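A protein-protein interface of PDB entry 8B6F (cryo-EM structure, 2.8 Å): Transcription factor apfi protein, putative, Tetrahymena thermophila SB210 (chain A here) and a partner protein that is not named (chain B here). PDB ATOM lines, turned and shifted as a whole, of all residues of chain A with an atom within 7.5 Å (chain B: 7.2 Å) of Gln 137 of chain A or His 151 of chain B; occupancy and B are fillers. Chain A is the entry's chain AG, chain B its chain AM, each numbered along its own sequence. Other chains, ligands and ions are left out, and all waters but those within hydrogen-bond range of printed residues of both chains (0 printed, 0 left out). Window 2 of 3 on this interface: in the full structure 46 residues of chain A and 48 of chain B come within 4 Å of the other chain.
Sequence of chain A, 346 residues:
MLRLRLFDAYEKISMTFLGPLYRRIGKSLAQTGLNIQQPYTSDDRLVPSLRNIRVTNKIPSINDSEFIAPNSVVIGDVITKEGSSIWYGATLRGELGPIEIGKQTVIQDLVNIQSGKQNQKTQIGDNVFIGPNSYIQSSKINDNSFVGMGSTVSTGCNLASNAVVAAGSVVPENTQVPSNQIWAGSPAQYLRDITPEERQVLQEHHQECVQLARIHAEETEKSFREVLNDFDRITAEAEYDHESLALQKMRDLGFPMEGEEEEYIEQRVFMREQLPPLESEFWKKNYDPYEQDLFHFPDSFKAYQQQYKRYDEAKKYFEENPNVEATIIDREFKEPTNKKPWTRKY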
ATOM      1  N   LEU A  96     -22.851  17.407   7.907  1.00  0.00           N
ATOM      2  CA  LEU A  96     -22.700  18.853   8.017  1.00  0.00           C
ATOM      3  C   LEU A  96     -23.157  19.543   6.739  1.00  0.00           C
ATOM      4  O   LEU A  96     -23.765  20.619   6.786  1.00  0.00           O
ATOM      5  CB  LEU A  96     -21.246  19.205   8.327  1.00  0.00           C
ATOM      6  CG  LEU A  96     -20.627  18.485   9.528  1.00  0.00           C
ATOM      7  CD1 LEU A  96     -19.213  18.979   9.773  1.00  0.00           C
ATOM      8  CD2 LEU A  96     -21.480  18.663  10.775  1.00  0.00           C
ATOM      9  N   PRO A  98     -23.822  18.533   2.119  1.00  0.00           N
ATOM     10  CA  PRO A  98     -23.624  17.574   1.026  1.00  0.00           C
ATOM     11  C   PRO A  98     -22.188  17.602   0.527  1.00  0.00           C
ATOM     12  O   PRO A  98     -21.570  18.662   0.419  1.00  0.00           O
ATOM     13  CB  PRO A  98     -24.608  18.050  -0.049  1.00  0.00           C
ATOM     14  CG  PRO A  98     -25.631  18.835   0.687  1.00  0.00           C
ATOM     15  CD  PRO A  98     -24.913  19.479   1.831  1.00  0.00           C
ATOM     16  N   ILE A  99     -21.660  16.421   0.221  1.00  0.00           N
ATOM     17  CA  ILE A  99     -20.306  16.264  -0.300  1.00  0.00           C
ATOM     18  C   ILE A  99     -20.415  15.559  -1.643  1.00  0.00           C
ATOM     19  O   ILE A  99     -20.706  14.358  -1.701  1.00  0.00           O
ATOM     20  CB  ILE A  99     -19.404  15.482   0.666  1.00  0.00           C
ATOM     21  CG1 ILE A  99     -19.123  16.321   1.915  1.00  0.00           C
ATOM     22  CG2 ILE A  99     -18.095  15.079  -0.018  1.00  0.00           C
ATOM     23  CD1 ILE A  99     -18.371  15.582   3.000  1.00  0.00           C
ATOM     24  N   ASN A 112      -9.651  15.067   5.250  1.00  0.00           N
ATOM     25  CA  ASN A 112     -10.907  15.351   5.928  1.00  0.00           C
ATOM     26  C   ASN A 112     -11.656  16.439   5.175  1.00  0.00           C
ATOM     27  O   ASN A 112     -11.073  17.469   4.827  1.00  0.00           O
ATOM     28  CB  ASN A 112     -10.666  15.796   7.372  1.00  0.00           C
ATOM     29  CG  ASN A 112     -10.123  14.689   8.241  1.00  0.00           C
ATOM     30  OD1 ASN A 112      -9.485  13.757   7.755  1.00  0.00           O
ATOM     31  ND2 ASN A 112     -10.378  14.781   9.539  1.00  0.00           N
ATOM     32  N   ILE A 113     -12.941  16.204   4.926  1.00  0.00           N
ATOM     33  CA  ILE A 113     -13.822  17.188   4.308  1.00  0.00           C
ATOM     34  C   ILE A 113     -14.961  17.441   5.284  1.00  0.00           C
ATOM     35  O   ILE A 113     -15.753  16.536   5.569  1.00  0.00           O
ATOM     36  CB  ILE A 113     -14.350  16.722   2.943  1.00  0.00           C
ATOM     37  CG1 ILE A 113     -13.181  16.262   2.064  1.00  0.00           C
ATOM     38  CG2 ILE A 113     -15.135  17.843   2.281  1.00  0.00           C
ATOM     39  CD1 ILE A 113     -13.552  15.895   0.634  1.00  0.00           C
ATOM     40  N   GLN A 114     -15.039  18.667   5.797  1.00  0.00           N
ATOM     41  CA  GLN A 114     -16.042  19.034   6.789  1.00  0.00           C
ATOM     42  C   GLN A 114     -16.488  20.463   6.531  1.00  0.00           C
ATOM     43  O   GLN A 114     -15.662  21.378   6.526  1.00  0.00           O
ATOM     44  CB  GLN A 114     -15.484  18.901   8.210  1.00  0.00           C
ATOM     45  CG  GLN A 114     -14.949  17.516   8.538  1.00  0.00           C
ATOM     46  CD  GLN A 114     -14.415  17.426   9.950  1.00  0.00           C
ATOM     47  OE1 GLN A 114     -14.564  18.353  10.744  1.00  0.00           O
ATOM     48  NE2 GLN A 114     -13.782  16.304  10.272  1.00  0.00           N
ATOM     49  N   SER A 115     -17.789  20.652   6.331  1.00  0.00           N
ATOM     50  CA  SER A 115     -18.339  21.979   6.078  1.00  0.00           C
ATOM     51  C   SER A 115     -18.429  22.754   7.385  1.00  0.00           C
ATOM     52  O   SER A 115     -19.077  22.305   8.336  1.00  0.00           O
ATOM     53  CB  SER A 115     -19.716  21.866   5.429  1.00  0.00           C
ATOM     54  OG  SER A 115     -19.646  21.160   4.202  1.00  0.00           O
ATOM     55  N   GLY A 116     -17.781  23.919   7.432  1.00  0.00           N
ATOM     56  CA  GLY A 116     -17.856  24.760   8.612  1.00  0.00           C
ATOM     57  C   GLY A 116     -19.205  25.415   8.809  1.00  0.00           C
ATOM     58  O   GLY A 116     -19.551  25.770   9.942  1.00  0.00           O
ATOM     59  N   LYS A 117     -19.975  25.584   7.737  1.00  0.00           N
ATOM     60  CA  LYS A 117     -21.313  26.139   7.832  1.00  0.00           C
ATOM     61  C   LYS A 117     -22.302  25.052   8.244  1.00  0.00           C
ATOM     62  O   LYS A 117     -21.960  23.873   8.369  1.00  0.00           O
ATOM     63  CB  LYS A 117     -21.716  26.779   6.506  1.00  0.00           C
ATOM     64  CG  LYS A 117     -20.886  27.997   6.118  1.00  0.00           C
ATOM     65  CD  LYS A 117     -21.124  29.152   7.084  1.00  0.00           C
ATOM     66  CE  LYS A 117     -20.411  30.420   6.638  1.00  0.00           C
ATOM     67  NZ  LYS A 117     -18.938  30.247   6.569  1.00  0.00           N
ATOM     68  N   GLN A 120     -23.863  24.232   4.196  1.00  0.00           N
ATOM     69  CA  GLN A 120     -23.155  24.506   2.954  1.00  0.00           C
ATOM     70  C   GLN A 120     -22.560  23.220   2.393  1.00  0.00           C
ATOM     71  O   GLN A 120     -22.000  22.404   3.129  1.00  0.00           O
ATOM     72  CB  GLN A 120     -22.062  25.548   3.185  1.00  0.00           C
ATOM     73  CG  GLN A 120     -21.398  26.036   1.909  1.00  0.00           C
ATOM     74  CD  GLN A 120     -22.352  26.763   0.988  1.00  0.00           C
ATOM     75  OE1 GLN A 120     -23.458  27.130   1.383  1.00  0.00           O
ATOM     76  NE2 GLN A 120     -21.926  26.975  -0.252  1.00  0.00           N
ATOM     77  N   LYS A 121     -22.681  23.042   1.081  1.00  0.00           N
ATOM     78  CA  LYS A 121     -22.248  21.819   0.423  1.00  0.00           C
ATOM     79  C   LYS A 121     -20.819  21.944  -0.092  1.00  0.00           C
ATOM     80  O   LYS A 121     -20.339  23.038  -0.400  1.00  0.00           O
ATOM     81  CB  LYS A 121     -23.181  21.474  -0.739  1.00  0.00           C
ATOM     82  CG  LYS A 121     -23.181  22.496  -1.864  1.00  0.00           C
ATOM     83  CD  LYS A 121     -24.115  22.076  -2.988  1.00  0.00           C
ATOM     84  CE  LYS A 121     -24.093  23.079  -4.133  1.00  0.00           C
ATOM     85  NZ  LYS A 121     -24.546  24.435  -3.711  1.00  0.00           N
ATOM     86  N   THR A 122     -20.142  20.802  -0.181  1.00  0.00           N
ATOM     87  CA  THR A 122     -18.806  20.706  -0.758  1.00  0.00           C
ATOM     88  C   THR A 122     -18.917  20.015  -2.110  1.00  0.00           C
ATOM     89  O   THR A 122     -19.341  18.858  -2.184  1.00  0.00           O
ATOM     90  CB  THR A 122     -17.862  19.928   0.159  1.00  0.00           C
ATOM     91  OG1 THR A 122     -17.814  20.553   1.449  1.00  0.00           O
ATOM     92  CG2 THR A 122     -16.457  19.884  -0.429  1.00  0.00           C
ATOM     93  N   TYR A 135      -7.160  19.184   3.804  1.00  0.00           N
ATOM     94  CA  TYR A 135      -8.332  19.546   4.597  1.00  0.00           C
ATOM     95  C   TYR A 135      -9.158  20.542   3.798  1.00  0.00           C
ATOM     96  O   TYR A 135      -8.786  21.713   3.692  1.00  0.00           O
ATOM     97  CB  TYR A 135      -7.919  20.130   5.945  1.00  0.00           C
ATOM     98  CG  TYR A 135      -9.081  20.433   6.861  1.00  0.00           C
ATOM     99  CD1 TYR A 135      -9.698  19.426   7.588  1.00  0.00           C
ATOM    100  CD2 TYR A 135      -9.554  21.728   7.006  1.00  0.00           C
ATOM    101  CE1 TYR A 135     -10.757  19.698   8.427  1.00  0.00           C
ATOM    102  CE2 TYR A 135     -10.613  22.009   7.843  1.00  0.00           C
ATOM    103  CZ  TYR A 135     -11.209  20.990   8.551  1.00  0.00           C
ATOM    104  OH  TYR A 135     -12.264  21.266   9.387  1.00  0.00           O
ATOM    105  N   ILE A 136     -10.274  20.078   3.245  1.00  0.00           N
ATOM    106  CA  ILE A 136     -11.201  20.919   2.500  1.00  0.00           C
ATOM    107  C   ILE A 136     -12.400  21.202   3.391  1.00  0.00           C
ATOM    108  O   ILE A 136     -13.032  20.271   3.902  1.00  0.00           O
ATOM    109  CB  ILE A 136     -11.644  20.237   1.193  1.00  0.00           C
ATOM    110  CG1 ILE A 136     -10.452  19.591   0.479  1.00  0.00           C
ATOM    111  CG2 ILE A 136     -12.341  21.234   0.282  1.00  0.00           C
ATOM    112  CD1 ILE A 136      -9.333  20.547   0.141  1.00  0.00           C
ATOM    113  N   GLN A 137     -12.723  22.481   3.583  1.00  0.00           N
ATOM    114  CA  GLN A 137     -13.834  22.823   4.465  1.00  0.00           C
ATOM    115  C   GLN A 137     -15.142  22.919   3.688  1.00  0.00           C
ATOM    116  O   GLN A 137     -16.060  22.119   3.895  1.00  0.00           O
ATOM    117  CB  GLN A 137     -13.563  24.148   5.185  1.00  0.00           C
ATOM    118  CG  GLN A 137     -12.598  24.051   6.342  1.00  0.00           C
ATOM    119  CD  GLN A 137     -12.489  25.356   7.101  1.00  0.00           C
ATOM    120  OE1 GLN A 137     -11.878  26.311   6.628  1.00  0.00           O
ATOM    121  NE2 GLN A 137     -13.090  25.404   8.284  1.00  0.00           N
ATOM    122  N   SER A 138     -15.230  23.882   2.781  1.00  0.00           N
ATOM    123  CA  SER A 138     -16.402  24.030   1.926  1.00  0.00           C
ATOM    124  C   SER A 138     -15.999  24.928   0.771  1.00  0.00           C
ATOM    125  O   SER A 138     -15.698  26.106   0.984  1.00  0.00           O
ATOM    126  CB  SER A 138     -17.563  24.618   2.707  1.00  0.00           C
ATOM    127  OG  SER A 138     -18.696  24.782   1.885  1.00  0.00           O
ATOM    128  N   SER A 139     -16.003  24.388  -0.443  1.00  0.00           N
ATOM    129  CA  SER A 139     -15.471  25.121  -1.581  1.00  0.00           C
ATOM    130  C   SER A 139     -16.011  24.517  -2.867  1.00  0.00           C
ATOM    131  O   SER A 139     -16.561  23.414  -2.881  1.00  0.00           O
ATOM    132  CB  SER A 139     -13.940  25.106  -1.570  1.00  0.00           C
ATOM    133  OG  SER A 139     -13.455  23.784  -1.419  1.00  0.00           O
ATOM    134  N   THR A 152      -4.733  23.090   2.873  1.00  0.00           N
ATOM    135  CA  THR A 152      -6.030  23.405   3.458  1.00  0.00           C
ATOM    136  C   THR A 152      -6.770  24.373   2.547  1.00  0.00           C
ATOM    137  O   THR A 152      -6.273  25.467   2.264  1.00  0.00           O
ATOM    138  CB  THR A 152      -5.871  24.002   4.859  1.00  0.00           C
ATOM    139  OG1 THR A 152      -5.269  23.032   5.724  1.00  0.00           O
ATOM    140  CG2 THR A 152      -7.221  24.414   5.431  1.00  0.00           C
ATOM    141  N   VAL A 153      -7.950  23.967   2.094  1.00  0.00           N
ATOM    142  CA  VAL A 153      -8.859  24.838   1.358  1.00  0.00           C
ATOM    143  C   VAL A 153      -9.942  25.283   2.330  1.00  0.00           C
ATOM    144  O   VAL A 153     -10.665  24.452   2.890  1.00  0.00           O
ATOM    145  CB  VAL A 153      -9.459  24.124   0.137  1.00  0.00           C
ATOM    146  CG1 VAL A 153     -10.401  25.050  -0.614  1.00  0.00           C
ATOM    147  CG2 VAL A 153      -8.357  23.628  -0.783  1.00  0.00           C
ATOM    148  N   SER A 154     -10.056  26.593   2.529  1.00  0.00           N
ATOM    149  CA  SER A 154     -10.930  27.141   3.551  1.00  0.00           C
ATOM    150  C   SER A 154     -12.351  27.298   3.016  1.00  0.00           C
ATOM    151  O   SER A 154     -12.638  27.038   1.846  1.00  0.00           O
ATOM    152  CB  SER A 154     -10.381  28.478   4.043  1.00  0.00           C
ATOM    153  OG  SER A 154      -9.123  28.310   4.672  1.00  0.00           O
ATOM    154  N   THR A 155     -13.256  27.730   3.889  1.00  0.00           N
ATOM    155  CA  THR A 155     -14.653  27.864   3.509  1.00  0.00           C
ATOM    156  C   THR A 155     -14.840  28.992   2.502  1.00  0.00           C
ATOM    157  O   THR A 155     -14.178  30.029   2.572  1.00  0.00           O
ATOM    158  CB  THR A 155     -15.512  28.125   4.745  1.00  0.00           C
ATOM    159  OG1 THR A 155     -15.409  27.020   5.650  1.00  0.00           O
ATOM    160  CG2 THR A 155     -16.971  28.316   4.362  1.00  0.00           C
ATOM    161  N   GLY A 156     -15.750  28.776   1.559  1.00  0.00           N
ATOM    162  CA  GLY A 156     -16.080  29.764   0.557  1.00  0.00           C
ATOM    163  C   GLY A 156     -15.080  29.896  -0.566  1.00  0.00           C
ATOM    164  O   GLY A 156     -15.241  30.786  -1.410  1.00  0.00           O
ATOM    165  N   CYS A 157     -14.053  29.053  -0.609  1.00  0.00           N
ATOM    166  CA  CYS A 157     -13.075  29.138  -1.680  1.00  0.00           C
ATOM    167  C   CYS A 157     -13.645  28.588  -2.981  1.00  0.00           C
ATOM    168  O   CYS A 157     -14.440  27.646  -2.988  1.00  0.00           O
ATOM    169  CB  CYS A 157     -11.817  28.354  -1.305  1.00  0.00           C
ATOM    170  SG  CYS A 157     -10.893  29.038   0.082  1.00  0.00           S
ATOM    171  N   VAL A 170      -1.995  27.013   2.642  1.00  0.00           N
ATOM    172  CA  VAL A 170      -3.240  27.300   3.346  1.00  0.00           C
ATOM    173  C   VAL A 170      -3.961  28.383   2.557  1.00  0.00           C
ATOM    174  O   VAL A 170      -3.573  29.556   2.594  1.00  0.00           O
ATOM    175  CB  VAL A 170      -2.989  27.738   4.794  1.00  0.00           C
ATOM    176  CG1 VAL A 170      -4.304  28.013   5.504  1.00  0.00           C
ATOM    177  CG2 VAL A 170      -2.188  26.682   5.535  1.00  0.00           C
ATOM    178  N   VAL A 171      -5.007  27.994   1.841  1.00  0.00           N
ATOM    179  CA  VAL A 171      -5.761  28.959   1.035  1.00  0.00           C
ATOM    180  C   VAL A 171      -6.603  29.834   1.961  1.00  0.00           C
ATOM    181  O   VAL A 171      -7.360  29.299   2.791  1.00  0.00           O
ATOM    182  CB  VAL A 171      -6.639  28.231   0.015  1.00  0.00           C
ATOM    183  CG1 VAL A 171      -7.361  29.230  -0.877  1.00  0.00           C
ATOM    184  CG2 VAL A 171      -5.802  27.276  -0.822  1.00  0.00           C
ATOM    185  N   GLU A 173      -9.615  32.013   3.535  1.00  0.00           N
ATOM    186  CA  GLU A 173     -11.057  31.863   3.425  1.00  0.00           C
ATOM    187  C   GLU A 173     -11.622  32.855   2.415  1.00  0.00           C
ATOM    188  O   GLU A 173     -11.193  34.010   2.348  1.00  0.00           O
ATOM    189  CB  GLU A 173     -11.710  32.067   4.793  1.00  0.00           C
ATOM    190  CG  GLU A 173     -13.172  31.664   4.852  1.00  0.00           C
ATOM    191  CD  GLU A 173     -13.763  31.828   6.236  1.00  0.00           C
ATOM    192  OE1 GLU A 173     -13.002  32.135   7.176  1.00  0.00           O
ATOM    193  OE2 GLU A 173     -14.990  31.647   6.386  1.00  0.00           O
ATOM    194  N   ILE B 132     -11.991  21.882  19.788  1.00  0.00           N
ATOM    195  CA  ILE B 132     -10.718  21.658  19.114  1.00  0.00           C
ATOM    196  C   ILE B 132     -11.013  21.129  17.718  1.00  0.00           C
ATOM    197  O   ILE B 132     -11.708  20.117  17.564  1.00  0.00           O
ATOM    198  CB  ILE B 132      -9.831  20.688  19.904  1.00  0.00           C
ATOM    199  CG1 ILE B 132      -9.748  21.155  21.360  1.00  0.00           C
ATOM    200  CG2 ILE B 132      -8.452  20.600  19.264  1.00  0.00           C
ATOM    201  CD1 ILE B 132      -8.826  20.354  22.232  1.00  0.00           C
ATOM    202  N   GLY B 133     -10.482  21.805  16.706  1.00  0.00           N
ATOM    203  CA  GLY B 133     -10.763  21.439  15.335  1.00  0.00           C
ATOM    204  C   GLY B 133     -10.060  20.163  14.918  1.00  0.00           C
ATOM    205  O   GLY B 133      -9.185  19.630  15.601  1.00  0.00           O
ATOM    206  N   ALA B 134     -10.464  19.662  13.755  1.00  0.00           N
ATOM    207  CA  ALA B 134      -9.880  18.443  13.219  1.00  0.00           C
ATOM    208  C   ALA B 134      -8.438  18.680  12.789  1.00  0.00           C
ATOM    209  O   ALA B 134      -8.075  19.757  12.312  1.00  0.00           O
ATOM    210  CB  ALA B 134     -10.702  17.936  12.034  1.00  0.00           C
ATOM    211  N   GLY B 135      -7.610  17.653  12.965  1.00  0.00           N
ATOM    212  CA  GLY B 135      -6.222  17.720  12.560  1.00  0.00           C
ATOM    213  C   GLY B 135      -5.303  18.440  13.518  1.00  0.00           C
ATOM    214  O   GLY B 135      -4.165  18.741  13.145  1.00  0.00           O
ATOM    215  N   CYS B 136      -5.756  18.731  14.734  1.00  0.00           N
ATOM    216  CA  CYS B 136      -4.922  19.412  15.712  1.00  0.00           C
ATOM    217  C   CYS B 136      -3.995  18.425  16.414  1.00  0.00           C
ATOM    218  O   CYS B 136      -4.252  17.221  16.478  1.00  0.00           O
ATOM    219  CB  CYS B 136      -5.788  20.124  16.751  1.00  0.00           C
ATOM    220  SG  CYS B 136      -6.733  21.514  16.112  1.00  0.00           S
ATOM    221  N   VAL B 149      -9.919  26.137  19.359  1.00  0.00           N
ATOM    222  CA  VAL B 149      -8.653  25.983  18.656  1.00  0.00           C
ATOM    223  C   VAL B 149      -8.966  25.596  17.218  1.00  0.00           C
ATOM    224  O   VAL B 149      -9.668  24.607  16.972  1.00  0.00           O
ATOM    225  CB  VAL B 149      -7.758  24.931  19.329  1.00  0.00           C
ATOM    226  CG1 VAL B 149      -6.406  24.870  18.650  1.00  0.00           C
ATOM    227  CG2 VAL B 149      -7.595  25.236  20.807  1.00  0.00           C
ATOM    228  N   GLY B 150      -8.446  26.371  16.271  1.00  0.00           N
ATOM    229  CA  GLY B 150      -8.742  26.128  14.878  1.00  0.00           C
ATOM    230  C   GLY B 150      -8.150  24.824  14.378  1.00  0.00           C
ATOM    231  O   GLY B 150      -7.272  24.223  14.996  1.00  0.00           O
ATOM    232  N   HIS B 151      -8.650  24.384  13.228  1.00  0.00           N
ATOM    233  CA  HIS B 151      -8.190  23.137  12.637  1.00  0.00           C
ATOM    234  C   HIS B 151      -6.720  23.239  12.247  1.00  0.00           C
ATOM    235  O   HIS B 151      -6.214  24.313  11.911  1.00  0.00           O
ATOM    236  CB  HIS B 151      -9.031  22.789  11.408  1.00  0.00           C
ATOM    237  CG  HIS B 151      -8.989  23.831  10.333  1.00  0.00           C
ATOM    238  ND1 HIS B 151      -9.954  24.808  10.205  1.00  0.00           N
ATOM    239  CD2 HIS B 151      -8.097  24.052   9.340  1.00  0.00           C
ATOM    240  CE1 HIS B 151      -9.658  25.583   9.178  1.00  0.00           C
ATOM    241  NE2 HIS B 151      -8.536  25.148   8.636  1.00  0.00           N
ATOM    242  N   ASN B 152      -6.030  22.099  12.296  1.00  0.00           N
ATOM    243  CA  ASN B 152      -4.620  22.016  11.914  1.00  0.00           C
ATOM    244  C   ASN B 152      -3.766  22.964  12.752  1.00  0.00           C
ATOM    245  O   ASN B 152      -2.937  23.714  12.234  1.00  0.00           O
ATOM    246  CB  ASN B 152      -4.442  22.298  10.422  1.00  0.00           C
ATOM    247  CG  ASN B 152      -5.134  21.276   9.550  1.00  0.00           C
ATOM    248  OD1 ASN B 152      -6.017  20.552  10.003  1.00  0.00           O
ATOM    249  ND2 ASN B 152      -4.736  21.212   8.285  1.00  0.00           N
ATOM    250  N   THR B 153      -3.971  22.919  14.064  1.00  0.00           N
ATOM    251  CA  THR B 153      -3.233  23.740  15.012  1.00  0.00           C
ATOM    252  C   THR B 153      -2.384  22.846  15.904  1.00  0.00           C
ATOM    253  O   THR B 153      -2.832  21.781  16.337  1.00  0.00           O
ATOM    254  CB  THR B 153      -4.181  24.590  15.868  1.00  0.00           C
ATOM    255  OG1 THR B 153      -4.713  25.661  15.080  1.00  0.00           O
ATOM    256  CG2 THR B 153      -3.461  25.178  17.082  1.00  0.00           C
ATOM    257  N   VAL B 154      -1.157  23.283  16.169  1.00  0.00           N
ATOM    258  CA  VAL B 154      -0.201  22.533  16.973  1.00  0.00           C
ATOM    259  C   VAL B 154       0.026  23.298  18.268  1.00  0.00           C
ATOM    260  O   VAL B 154       0.346  24.492  18.244  1.00  0.00           O
ATOM    261  CB  VAL B 154       1.122  22.314  16.219  1.00  0.00           C
ATOM    262  CG1 VAL B 154       2.092  21.498  17.062  1.00  0.00           C
ATOM    263  CG2 VAL B 154       0.866  21.624  14.892  1.00  0.00           C
ATOM    264  N   ILE B 167      -7.655  30.639  18.774  1.00  0.00           N
ATOM    265  CA  ILE B 167      -6.477  30.441  17.943  1.00  0.00           C
ATOM    266  C   ILE B 167      -6.955  30.110  16.537  1.00  0.00           C
ATOM    267  O   ILE B 167      -7.729  29.165  16.344  1.00  0.00           O
ATOM    268  CB  ILE B 167      -5.567  29.339  18.504  1.00  0.00           C
ATOM    269  CG1 ILE B 167      -5.070  29.742  19.893  1.00  0.00           C
ATOM    270  CG2 ILE B 167      -4.394  29.078  17.571  1.00  0.00           C
ATOM    271  CD1 ILE B 167      -4.368  28.641  20.627  1.00  0.00           C
ATOM    272  N   ALA B 168      -6.498  30.886  15.562  1.00  0.00           N
ATOM    273  CA  ALA B 168      -6.901  30.665  14.188  1.00  0.00           C
ATOM    274  C   ALA B 168      -6.334  29.341  13.680  1.00  0.00           C
ATOM    275  O   ALA B 168      -5.298  28.876  14.158  1.00  0.00           O
ATOM    276  CB  ALA B 168      -6.425  31.807  13.298  1.00  0.00           C
ATOM    277  N   PRO B 169      -6.994  28.714  12.710  1.00  0.00           N
ATOM    278  CA  PRO B 169      -6.494  27.440  12.186  1.00  0.00           C
ATOM    279  C   PRO B 169      -5.177  27.616  11.446  1.00  0.00           C
ATOM    280  O   PRO B 169      -4.841  28.695  10.954  1.00  0.00           O
ATOM    281  CB  PRO B 169      -7.607  26.982  11.239  1.00  0.00           C
ATOM    282  CG  PRO B 169      -8.303  28.232  10.845  1.00  0.00           C
ATOM    283  CD  PRO B 169      -8.232  29.138  12.034  1.00  0.00           C
ATOM    284  N   ASN B 170      -4.422  26.519  11.379  1.00  0.00           N
ATOM    285  CA  ASN B 170      -3.133  26.489  10.688  1.00  0.00           C
ATOM    286  C   ASN B 170      -2.099  27.353  11.405  1.00  0.00           C
ATOM    287  O   ASN B 170      -1.274  28.014  10.774  1.00  0.00           O
ATOM    288  CB  ASN B 170      -3.283  26.920   9.228  1.00  0.00           C
ATOM    289  CG  ASN B 170      -4.356  26.141   8.504  1.00  0.00           C
ATOM    290  OD1 ASN B 170      -5.356  26.702   8.060  1.00  0.00           O
ATOM    291  ND2 ASN B 170      -4.155  24.837   8.383  1.00  0.00           N
ATOM    292  N   SER B 171      -2.147  27.348  12.733  1.00  0.00           N
ATOM    293  CA  SER B 171      -1.223  28.099  13.567  1.00  0.00           C
ATOM    294  C   SER B 171      -0.641  27.175  14.625  1.00  0.00           C
ATOM    295  O   SER B 171      -1.249  26.166  14.988  1.00  0.00           O
ATOM    296  CB  SER B 171      -1.917  29.293  14.231  1.00  0.00           C
ATOM    297  OG  SER B 171      -3.095  28.890  14.899  1.00  0.00           O
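The side-chain hydroxyl (OG1) of Thr 152 of chain A sits at hydrogen-bond distance from the side-chain amide nitrogen (ND2) of Asn 152 of chain B (3.2 Å).
The side-chain hydroxyl (OG1) of Thr 152 of chain A sits at hydrogen-bond distance from the side-chain amide nitrogen (ND2) of Asn 170 of chain B, at 3.4 Å.
The backbone NH of Val 171 of chain A sits at hydrogen-bond distance from the backbone carbonyl oxygen of Thr 152 of chain A (2.9 Å).
O of Ala 134 of chain B sits at hydrogen-bond distance from N of Asn 152 of chain B (3.1 Å).
The side-chain amide oxygen (OE1) of Gln 137 of chain A lies within hydrogen-bond range of the backbone NH (N) of Thr 155 of chain A (3.4 Å).
The backbone carbonyl oxygen (O) of His 151 of chain B lies within hydrogen-bond range of the backbone NH (N) of Asn 170 of chain B, 2.9 Å away.
O of Tyr 135 of chain A is in hydrogen-bond range of N of Val 153 of chain A (2.9 Å).
The backbone carbonyl oxygen (O) of Gln 137 of chain A sits close to the backbone NH (N) of Ser 115 of chain A.
Among the printed residues, pairs that only touch across the chains: Gln 114 of chain A with Ala 134 of chain B, Tyr 135 of chain A with His 151 of chain B, Gln 137 of chain A with His 151 of chain B, Thr 152 of chain A with His 151 of chain B and Val 170 of chain A with Asn 170 of chain B.
Gly 116 of chain A touches none of the printed residues of chain B.
Thr 122 of chain A touches none of the printed residues of chain B.
Of the printed residues of chain B, Tyr 135 of chain A touches His 151.
Gln 137 of chain A touches just one residue of chain B: His 151.
Of the printed residues of chain B, Thr 152 of chain A touches His 151 (3.5 Å), Asn 152 (3.2 Å) and Asn 170 (3.4 Å).
Printed residues of chain B within 4 Å of Val 170 of chain A: Asn 170 (3.1 Å).
His 151 of chain B touches just these residues of chain A: Tyr 135 (3.5 Å), Gln 137 (3.5 Å) and Thr 152 (3.5 Å).
Of the printed residues of chain A, Asn 152 of chain B touches Thr 152.
The nearest residue of chain B that does not touch Gln 137 of chain A is Pro 169 of chain B (5.9 Å).
The nearest residue of chain A that does not touch His 151 of chain B is Ser 154 of chain A (5.1 Å).
The nearest printed residue of chain A that does not touch Ala 134 of chain B is Tyr 135 of chain A (4.01 Å).
Printed residues of chain B that touch a printed residue of chain A: Ala 134, His 151, Asn 152 and Asn 170.
Hydrophobic or aromatic side chains of chain B within 4 Å of the printed part of chain A: Ala 134 and His 151.
Along chain B the printed residues that touch a printed residue of chain A span positions 134 to 170.
Of the 26 printed residues of chain A, 5 touch a printed residue of chain B.
Among the printed residues, no Asp or Glu carboxylate lies within 4 Å of a Lys or Arg side-chain nitrogen of the other chain.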
